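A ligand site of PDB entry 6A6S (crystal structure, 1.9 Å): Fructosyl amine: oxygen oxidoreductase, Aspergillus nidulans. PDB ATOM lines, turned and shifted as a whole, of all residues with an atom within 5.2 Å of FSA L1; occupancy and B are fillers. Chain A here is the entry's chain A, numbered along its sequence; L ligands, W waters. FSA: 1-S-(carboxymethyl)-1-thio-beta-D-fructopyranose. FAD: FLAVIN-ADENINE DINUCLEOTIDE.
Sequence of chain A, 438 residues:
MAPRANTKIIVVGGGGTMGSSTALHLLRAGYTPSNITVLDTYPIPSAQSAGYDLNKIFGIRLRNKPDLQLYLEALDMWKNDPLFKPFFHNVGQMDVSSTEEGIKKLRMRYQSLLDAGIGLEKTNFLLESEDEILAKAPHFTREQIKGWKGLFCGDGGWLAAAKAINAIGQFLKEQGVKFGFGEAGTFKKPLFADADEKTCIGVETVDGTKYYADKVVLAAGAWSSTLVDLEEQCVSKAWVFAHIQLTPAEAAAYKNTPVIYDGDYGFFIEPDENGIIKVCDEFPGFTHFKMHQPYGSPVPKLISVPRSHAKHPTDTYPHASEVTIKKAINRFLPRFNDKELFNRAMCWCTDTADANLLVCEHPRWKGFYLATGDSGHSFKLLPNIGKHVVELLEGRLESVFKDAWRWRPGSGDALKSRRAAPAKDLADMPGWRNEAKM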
ATOM      1  N   ILE A  57       3.590 -16.667  -9.527  1.00  0.00           N
ATOM      2  CA  ILE A  57       4.861 -16.057  -9.207  1.00  0.00           C
ATOM      3  C   ILE A  57       5.838 -15.991 -10.370  1.00  0.00           C
ATOM      4  O   ILE A  57       5.970 -16.930 -11.080  1.00  0.00           O
ATOM      5  CB  ILE A  57       5.531 -16.821  -8.057  1.00  0.00           C
ATOM      6  CG1 ILE A  57       4.611 -16.889  -6.875  1.00  0.00           C
ATOM      7  CG2 ILE A  57       6.824 -16.166  -7.695  1.00  0.00           C
ATOM      8  CD1 ILE A  57       5.127 -17.742  -5.760  1.00  0.00           C
ATOM      9  N   GLY A  59       9.876 -15.541 -10.785  1.00  0.00           N
ATOM     10  CA  GLY A  59      11.076 -15.549 -10.002  1.00  0.00           C
ATOM     11  C   GLY A  59      12.123 -16.419 -10.641  1.00  0.00           C
ATOM     12  O   GLY A  59      11.879 -17.159 -11.550  1.00  0.00           O
ATOM     13  N   ARG A  61      14.614 -19.462 -10.797  1.00  0.00           N
ATOM     14  CA  ARG A  61      14.791 -20.779 -10.214  1.00  0.00           C
ATOM     15  C   ARG A  61      15.710 -21.615 -11.087  1.00  0.00           C
ATOM     16  O   ARG A  61      15.298 -22.110 -12.136  1.00  0.00           O
ATOM     17  CB  ARG A  61      13.429 -21.460 -10.028  1.00  0.00           C
ATOM     18  CG  ARG A  61      13.503 -22.896  -9.551  1.00  0.00           C
ATOM     19  CD  ARG A  61      12.141 -23.462  -9.163  1.00  0.00           C
ATOM     20  NE  ARG A  61      12.230 -24.893  -8.854  1.00  0.00           N
ATOM     21  CZ  ARG A  61      11.568 -25.508  -7.885  1.00  0.00           C
ATOM     22  NH1 ARG A  61      10.753 -24.826  -7.098  1.00  0.00           N
ATOM     23  NH2 ARG A  61      11.733 -26.814  -7.684  1.00  0.00           N
ATOM     24  N   TRP A 239      -2.040 -29.290  -7.462  1.00  0.00           N
ATOM     25  CA  TRP A 239      -1.707 -28.444  -6.318  1.00  0.00           C
ATOM     26  C   TRP A 239      -2.961 -27.679  -5.918  1.00  0.00           C
ATOM     27  O   TRP A 239      -3.981 -27.719  -6.621  1.00  0.00           O
ATOM     28  CB  TRP A 239      -0.525 -27.532  -6.629  1.00  0.00           C
ATOM     29  CG  TRP A 239       0.743 -28.289  -6.443  1.00  0.00           C
ATOM     30  CD1 TRP A 239       1.520 -28.344  -5.310  1.00  0.00           C
ATOM     31  CD2 TRP A 239       1.337 -29.191  -7.388  1.00  0.00           C
ATOM     32  NE1 TRP A 239       2.580 -29.191  -5.509  1.00  0.00           N
ATOM     33  CE2 TRP A 239       2.492 -29.720  -6.773  1.00  0.00           C
ATOM     34  CE3 TRP A 239       1.020 -29.577  -8.702  1.00  0.00           C
ATOM     35  CZ2 TRP A 239       3.327 -30.636  -7.429  1.00  0.00           C
ATOM     36  CZ3 TRP A 239       1.854 -30.470  -9.350  1.00  0.00           C
ATOM     37  CH2 TRP A 239       2.993 -30.991  -8.722  1.00  0.00           C
ATOM     38  N   TYR A 261       7.421 -16.527   0.277  1.00  0.00           N
ATOM     39  CA  TYR A 261       7.483 -17.987   0.202  1.00  0.00           C
ATOM     40  C   TYR A 261       8.331 -18.595   1.333  1.00  0.00           C
ATOM     41  O   TYR A 261       9.360 -18.038   1.663  1.00  0.00           O
ATOM     42  CB  TYR A 261       8.062 -18.426  -1.154  1.00  0.00           C
ATOM     43  CG  TYR A 261       8.172 -19.934  -1.347  1.00  0.00           C
ATOM     44  CD1 TYR A 261       9.336 -20.615  -1.045  1.00  0.00           C
ATOM     45  CD2 TYR A 261       7.118 -20.667  -1.897  1.00  0.00           C
ATOM     46  CE1 TYR A 261       9.457 -21.998  -1.236  1.00  0.00           C
ATOM     47  CE2 TYR A 261       7.214 -22.054  -2.093  1.00  0.00           C
ATOM     48  CZ  TYR A 261       8.385 -22.700  -1.766  1.00  0.00           C
ATOM     49  OH  TYR A 261       8.477 -24.066  -1.964  1.00  0.00           O
ATOM     50  N   PHE A 267       2.996 -20.096   0.219  1.00  0.00           N
ATOM     51  CA  PHE A 267       3.178 -18.700  -0.125  1.00  0.00           C
ATOM     52  C   PHE A 267       1.863 -17.966  -0.235  1.00  0.00           C
ATOM     53  O   PHE A 267       0.806 -18.589  -0.302  1.00  0.00           O
ATOM     54  CB  PHE A 267       3.977 -18.570  -1.443  1.00  0.00           C
ATOM     55  CG  PHE A 267       3.285 -19.173  -2.652  1.00  0.00           C
ATOM     56  CD1 PHE A 267       3.567 -20.467  -3.058  1.00  0.00           C
ATOM     57  CD2 PHE A 267       2.374 -18.423  -3.393  1.00  0.00           C
ATOM     58  CE1 PHE A 267       2.947 -21.024  -4.196  1.00  0.00           C
ATOM     59  CE2 PHE A 267       1.744 -18.977  -4.530  1.00  0.00           C
ATOM     60  CZ  PHE A 267       2.040 -20.272  -4.919  1.00  0.00           C
ATOM     61  N   CYS A 280      -1.261 -20.548  -1.261  1.00  0.00           N
ATOM     62  CA  CYS A 280      -0.926 -21.925  -1.576  1.00  0.00           C
ATOM     63  C   CYS A 280      -0.108 -22.525  -0.450  1.00  0.00           C
ATOM     64  O   CYS A 280       0.671 -21.831   0.189  1.00  0.00           O
ATOM     65  CB  CYS A 280      -0.135 -22.030  -2.859  1.00  0.00           C
ATOM     66  SG  CYS A 280      -1.038 -21.632  -4.373  1.00  0.00           S
ATOM     67  N   ASP A 281      -0.229 -23.828  -0.235  1.00  0.00           N
ATOM     68  CA  ASP A 281       0.741 -24.504   0.638  1.00  0.00           C
ATOM     69  C   ASP A 281       1.911 -24.986  -0.215  1.00  0.00           C
ATOM     70  O   ASP A 281       2.014 -24.626  -1.374  1.00  0.00           O
ATOM     71  CB  ASP A 281       0.086 -25.661   1.410  1.00  0.00           C
ATOM     72  CG  ASP A 281      -0.494 -26.727   0.497  1.00  0.00           C
ATOM     73  OD1 ASP A 281      -0.554 -26.524  -0.737  1.00  0.00           O
ATOM     74  OD2 ASP A 281      -0.903 -27.783   1.024  1.00  0.00           O
ATOM     75  N   GLU A 282       2.786 -25.789   0.366  1.00  0.00           N
ATOM     76  CA  GLU A 282       3.846 -26.423  -0.400  1.00  0.00           C
ATOM     77  C   GLU A 282       3.877 -27.899  -0.031  1.00  0.00           C
ATOM     78  O   GLU A 282       4.055 -28.257   1.135  1.00  0.00           O
ATOM     79  CB  GLU A 282       5.204 -25.784  -0.125  1.00  0.00           C
ATOM     80  CG  GLU A 282       6.355 -26.371  -0.949  1.00  0.00           C
ATOM     81  CD  GLU A 282       6.133 -26.209  -2.462  1.00  0.00           C
ATOM     82  OE1 GLU A 282       5.395 -27.025  -3.063  1.00  0.00           O
ATOM     83  OE2 GLU A 282       6.693 -25.250  -3.041  1.00  0.00           O
ATOM     84  N   PHE A 283       3.699 -28.742  -1.035  1.00  0.00           N
ATOM     85  CA  PHE A 283       3.671 -30.179  -0.824  1.00  0.00           C
ATOM     86  C   PHE A 283       3.935 -30.846  -2.191  1.00  0.00           C
ATOM     87  O   PHE A 283       4.052 -30.149  -3.191  1.00  0.00           O
ATOM     88  CB  PHE A 283       2.343 -30.612  -0.203  1.00  0.00           C
ATOM     89  CG  PHE A 283       1.189 -30.646  -1.177  1.00  0.00           C
ATOM     90  CD1 PHE A 283       0.769 -29.497  -1.847  1.00  0.00           C
ATOM     91  CD2 PHE A 283       0.517 -31.845  -1.419  1.00  0.00           C
ATOM     92  CE1 PHE A 283      -0.297 -29.557  -2.765  1.00  0.00           C
ATOM     93  CE2 PHE A 283      -0.556 -31.900  -2.326  1.00  0.00           C
ATOM     94  CZ  PHE A 283      -0.956 -30.756  -2.990  1.00  0.00           C
ATOM     95  N   CYS A 349      -0.806 -29.850 -13.038  1.00  0.00           N
ATOM     96  CA  CYS A 349       0.426 -29.780 -13.805  1.00  0.00           C
ATOM     97  C   CYS A 349       0.894 -31.192 -14.093  1.00  0.00           C
ATOM     98  O   CYS A 349       0.289 -32.144 -13.598  1.00  0.00           O
ATOM     99  CB  CYS A 349       1.510 -29.013 -13.039  1.00  0.00           C
ATOM    100  SG  CYS A 349       0.995 -27.375 -12.491  1.00  0.00           S
ATOM    101  N   SER A 375       5.997 -29.272 -15.436  1.00  0.00           N
ATOM    102  CA  SER A 375       6.581 -29.560 -14.113  1.00  0.00           C
ATOM    103  C   SER A 375       6.290 -28.497 -13.031  1.00  0.00           C
ATOM    104  O   SER A 375       7.050 -28.357 -12.065  1.00  0.00           O
ATOM    105  CB  SER A 375       8.075 -29.782 -14.258  1.00  0.00           C
ATOM    106  OG  SER A 375       8.312 -30.947 -15.034  1.00  0.00           O
ATOM    107  N   GLY A 376       5.170 -27.798 -13.181  1.00  0.00           N
ATOM    108  CA  GLY A 376       4.658 -26.924 -12.148  1.00  0.00           C
ATOM    109  C   GLY A 376       5.410 -25.613 -11.969  1.00  0.00           C
ATOM    110  O   GLY A 376       5.185 -24.901 -11.000  1.00  0.00           O
ATOM    111  N   HIS A 377       6.281 -25.280 -12.917  1.00  0.00           N
ATOM    112  CA  HIS A 377       7.064 -24.066 -12.805  1.00  0.00           C
ATOM    113  C   HIS A 377       7.165 -23.278 -14.114  1.00  0.00           C
ATOM    114  O   HIS A 377       8.106 -22.513 -14.298  1.00  0.00           O
ATOM    115  CB  HIS A 377       8.483 -24.405 -12.328  1.00  0.00           C
ATOM    116  CG  HIS A 377       8.532 -25.178 -11.044  1.00  0.00           C
ATOM    117  ND1 HIS A 377       8.230 -24.605  -9.822  1.00  0.00           N
ATOM    118  CD2 HIS A 377       8.875 -26.462 -10.783  1.00  0.00           C
ATOM    119  CE1 HIS A 377       8.366 -25.515  -8.871  1.00  0.00           C
ATOM    120  NE2 HIS A 377       8.759 -26.651  -9.427  1.00  0.00           N
ATOM    121  N   LYS A 380       5.675 -18.829 -15.815  1.00  0.00           N
ATOM    122  CA  LYS A 380       6.592 -17.718 -16.010  1.00  0.00           C
ATOM    123  C   LYS A 380       7.124 -17.673 -17.461  1.00  0.00           C
ATOM    124  O   LYS A 380       7.579 -16.624 -17.904  1.00  0.00           O
ATOM    125  CB  LYS A 380       7.763 -17.810 -15.002  1.00  0.00           C
ATOM    126  CG  LYS A 380       8.639 -19.039 -15.150  1.00  0.00           C
ATOM    127  CD  LYS A 380       9.707 -19.166 -14.052  1.00  0.00           C
ATOM    128  CE  LYS A 380       9.064 -19.430 -12.690  1.00  0.00           C
ATOM    129  NZ  LYS A 380      10.063 -19.874 -11.678  1.00  0.00           N
ATOM    130  N   ARG A 419      10.744 -33.474  -6.328  1.00  0.00           N
ATOM    131  CA  ARG A 419      10.036 -33.080  -5.123  1.00  0.00           C
ATOM    132  C   ARG A 419      10.415 -33.963  -3.941  1.00  0.00           C
ATOM    133  O   ARG A 419      11.208 -34.900  -4.089  1.00  0.00           O
ATOM    134  CB  ARG A 419       8.537 -33.130  -5.384  1.00  0.00           C
ATOM    135  CG  ARG A 419       8.174 -32.416  -6.691  1.00  0.00           C
ATOM    136  CD  ARG A 419       6.704 -32.034  -6.770  1.00  0.00           C
ATOM    137  NE  ARG A 419       6.407 -31.365  -8.044  1.00  0.00           N
ATOM    138  CZ  ARG A 419       6.349 -30.043  -8.221  1.00  0.00           C
ATOM    139  NH1 ARG A 419       6.528 -29.216  -7.184  1.00  0.00           N
ATOM    140  NH2 ARG A 419       6.087 -29.562  -9.426  1.00  0.00           N
HETATM  141  OAB FSA L   1       8.120 -21.721 -10.291  1.00  0.00           O
HETATM  142  CAL FSA L   1       8.019 -20.850  -9.403  1.00  0.00           C
HETATM  143  OAA FSA L   1       8.701 -19.795  -9.433  1.00  0.00           O
HETATM  144  CAH FSA L   1       6.950 -21.013  -8.330  1.00  0.00           C
HETATM  145  SAK FSA L   1       5.791 -22.292  -8.740  1.00  0.00           S
HETATM  146  C1  FSA L   1       4.611 -22.286  -7.416  1.00  0.00           C
HETATM  147  C2  FSA L   1       3.940 -23.651  -7.223  1.00  0.00           C
HETATM  148  O2  FSA L   1       2.705 -23.516  -6.493  1.00  0.00           O
HETATM  149  C3  FSA L   1       4.883 -24.558  -6.425  1.00  0.00           C
HETATM  150  O3  FSA L   1       5.128 -24.026  -5.126  1.00  0.00           O
HETATM  151  C4  FSA L   1       4.351 -25.981  -6.308  1.00  0.00           C
HETATM  152  O4  FSA L   1       5.400 -26.805  -5.784  1.00  0.00           O
HETATM  153  C5  FSA L   1       3.920 -26.514  -7.679  1.00  0.00           C
HETATM  154  O5  FSA L   1       5.085 -26.728  -8.474  1.00  0.00           O
HETATM  155  C6  FSA L   1       3.000 -25.530  -8.378  1.00  0.00           C
HETATM  156  O6  FSA L   1       3.659 -24.273  -8.492  1.00  0.00           O
HETATM  157  PA  FAD L   2      -2.096 -25.668 -19.249  1.00  0.00           P
HETATM  158  O1A FAD L   2      -1.912 -24.256 -19.203  1.00  0.00           O
HETATM  159  O2A FAD L   2      -2.994 -26.255 -18.333  1.00  0.00           O
HETATM  160  O5B FAD L   2      -2.704 -25.951 -20.645  1.00  0.00           O
HETATM  161  C5B FAD L   2      -3.278 -27.173 -21.010  1.00  0.00           C
HETATM  162  C4B FAD L   2      -4.470 -26.939 -21.928  1.00  0.00           C
HETATM  163  O4B FAD L   2      -4.820 -28.105 -22.632  1.00  0.00           O
HETATM  164  C3B FAD L   2      -5.706 -26.517 -21.207  1.00  0.00           C
HETATM  165  O3B FAD L   2      -6.108 -25.309 -21.765  1.00  0.00           O
HETATM  166  C2B FAD L   2      -6.696 -27.626 -21.472  1.00  0.00           C
HETATM  167  O2B FAD L   2      -7.998 -27.182 -21.679  1.00  0.00           O
HETATM  168  C1B FAD L   2      -6.199 -28.178 -22.773  1.00  0.00           C
HETATM  169  N9A FAD L   2      -6.642 -29.560 -23.002  1.00  0.00           N
HETATM  170  C8A FAD L   2      -6.720 -30.526 -22.118  1.00  0.00           C
HETATM  171  N7A FAD L   2      -7.161 -31.658 -22.682  1.00  0.00           N
HETATM  172  C5A FAD L   2      -7.356 -31.414 -23.963  1.00  0.00           C
HETATM  173  C6A FAD L   2      -7.830 -32.142 -25.153  1.00  0.00           C
HETATM  174  N6A FAD L   2      -8.158 -33.427 -25.049  1.00  0.00           N
HETATM  175  N1A FAD L   2      -7.892 -31.509 -26.311  1.00  0.00           N
HETATM  176  C2A FAD L   2      -7.565 -30.233 -26.404  1.00  0.00           C
HETATM  177  N3A FAD L   2      -7.149 -29.513 -25.396  1.00  0.00           N
HETATM  178  C4A FAD L   2      -7.012 -30.027 -24.168  1.00  0.00           C
HETATM  179  N1  FAD L   2       4.229 -21.445 -12.461  1.00  0.00           N
HETATM  180  C2  FAD L   2       5.006 -20.385 -12.275  1.00  0.00           C
HETATM  181  O2  FAD L   2       5.828 -20.131 -13.108  1.00  0.00           O
HETATM  182  N3  FAD L   2       4.890 -19.629 -11.192  1.00  0.00           N
HETATM  183  C4  FAD L   2       3.998 -19.870 -10.242  1.00  0.00           C
HETATM  184  O4  FAD L   2       3.855 -19.186  -9.236  1.00  0.00           O
HETATM  185  C4X FAD L   2       3.106 -21.006 -10.391  1.00  0.00           C
HETATM  186  N5  FAD L   2       2.191 -21.307  -9.510  1.00  0.00           N
HETATM  187  C5X FAD L   2       1.390 -22.341  -9.705  1.00  0.00           C
HETATM  188  C6  FAD L   2       0.444 -22.625  -8.788  1.00  0.00           C
HETATM  189  C7  FAD L   2      -0.403 -23.658  -8.941  1.00  0.00           C
HETATM  190  C7M FAD L   2      -1.439 -23.948  -7.920  1.00  0.00           C
HETATM  191  C8  FAD L   2      -0.291 -24.497 -10.125  1.00  0.00           C
HETATM  192  C8M FAD L   2      -1.238 -25.620 -10.243  1.00  0.00           C
HETATM  193  C9  FAD L   2       0.675 -24.233 -11.065  1.00  0.00           C
HETATM  194  C9A FAD L   2       1.532 -23.179 -10.896  1.00  0.00           C
HETATM  195  N10 FAD L   2       2.499 -22.860 -11.822  1.00  0.00           N
HETATM  196  C10 FAD L   2       3.285 -21.786 -11.609  1.00  0.00           C
HETATM  197  C1' FAD L   2       2.701 -23.659 -12.991  1.00  0.00           C
HETATM  198  C2' FAD L   2       1.905 -23.304 -14.193  1.00  0.00           C
HETATM  199  O2' FAD L   2       0.573 -23.097 -13.834  1.00  0.00           O
HETATM  200  C3' FAD L   2       2.017 -24.474 -15.177  1.00  0.00           C
HETATM  201  O3' FAD L   2       3.314 -24.957 -15.273  1.00  0.00           O
HETATM  202  C4' FAD L   2       1.633 -24.028 -16.577  1.00  0.00           C
HETATM  203  O4' FAD L   2       0.596 -23.115 -16.547  1.00  0.00           O
HETATM  204  C5' FAD L   2       1.232 -25.230 -17.430  1.00  0.00           C
HETATM  205  O5' FAD L   2       1.199 -24.904 -18.801  1.00  0.00           O
HETATM  206  P   FAD L   2       0.588 -25.924 -19.796  1.00  0.00           P
HETATM  207  O1P FAD L   2       1.467 -27.061 -19.802  1.00  0.00           O
HETATM  208  O2P FAD L   2       0.272 -25.263 -20.983  1.00  0.00           O
HETATM  209  O3P FAD L   2      -0.724 -26.404 -19.173  1.00  0.00           O
HETATM  210  O   HOH W   1       1.665 -24.783  -4.222  1.00  0.00           O
HETATM  211  O   HOH W   2       6.720 -29.513  -4.239  1.00  0.00           O
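SAK of FSA L1 sits close to N3 of FAD L2, at 3.7 Å.
The side-chain amino group (NZ) of Lys 380 lies within hydrogen-bond range of the backbone carbonyl oxygen (O) of Gly 59, 3.3 Å away. The guanidinium group of Arg 61 lies close to a ring nitrogen (NE2) of His 377, at 3.5 Å. N of Phe 267 lies within hydrogen-bond range of O of Cys 280. NH2 of Arg 419 sits at hydrogen-bond distance from O of Ser 375 (3.1 Å). The backbone carbonyl oxygen of Phe 283 is in hydrogen-bond range of the indole nitrogen of Trp 239.
Water W1 bridges an oxygen (O2) of FSA L1 (2.8 Å) and the backbone carbonyl oxygen of Asp 281 (2.9 Å). Water W2 lies within hydrogen-bond range of O of Phe 283 (2.9 Å), NH1 of Arg 419 (3.0 Å), OE1 of Glu 282 (3.1 Å) and O4 of FSA L1 (3.4 Å).
The side-chain carboxylate of Glu 282 sits at hydrogen-bond distance from an oxygen (O4) of FSA L1, 2.7 Å away. The side-chain amino group (NZ) of Lys 380 is in salt-bridge range of an oxygen (OAA) of FSA L1 (2.6 Å). The backbone carbonyl oxygen of Ile 57 is in hydrogen-bond range of a nitrogen (N3) of FAD L2 (2.9 Å). N of Ile 57 is in hydrogen-bond range of O4 of FAD L2, 2.5 Å away. ND1 of His 377 is in hydrogen-bond range of OAB of FSA L1. O4 of FSA L1 lies within hydrogen-bond range of NH1 of Arg 419 (3.0 Å). An oxygen (O2) of FAD L2 is in hydrogen-bond range of the backbone NH (N) of Lys 380 (3.0 Å). The backbone carbonyl oxygen (O) of Gly 376 lies within hydrogen-bond range of an oxygen (O5) of FSA L1 (3.1 Å).
Trp 239 touches FSA L1 (CE2 to C5, 3.6 Å). CE1 of Phe 267 touches O2 of FSA L1 (3.4 Å). Hydrophobic or aromatic side chains within 4 Å of FSA L1: Trp 239, Phe 267 and His 377. Within 4 Å of FSA L1: Trp 239, Phe 267, Glu 282, Gly 376, His 377, Lys 380 and Arg 419.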
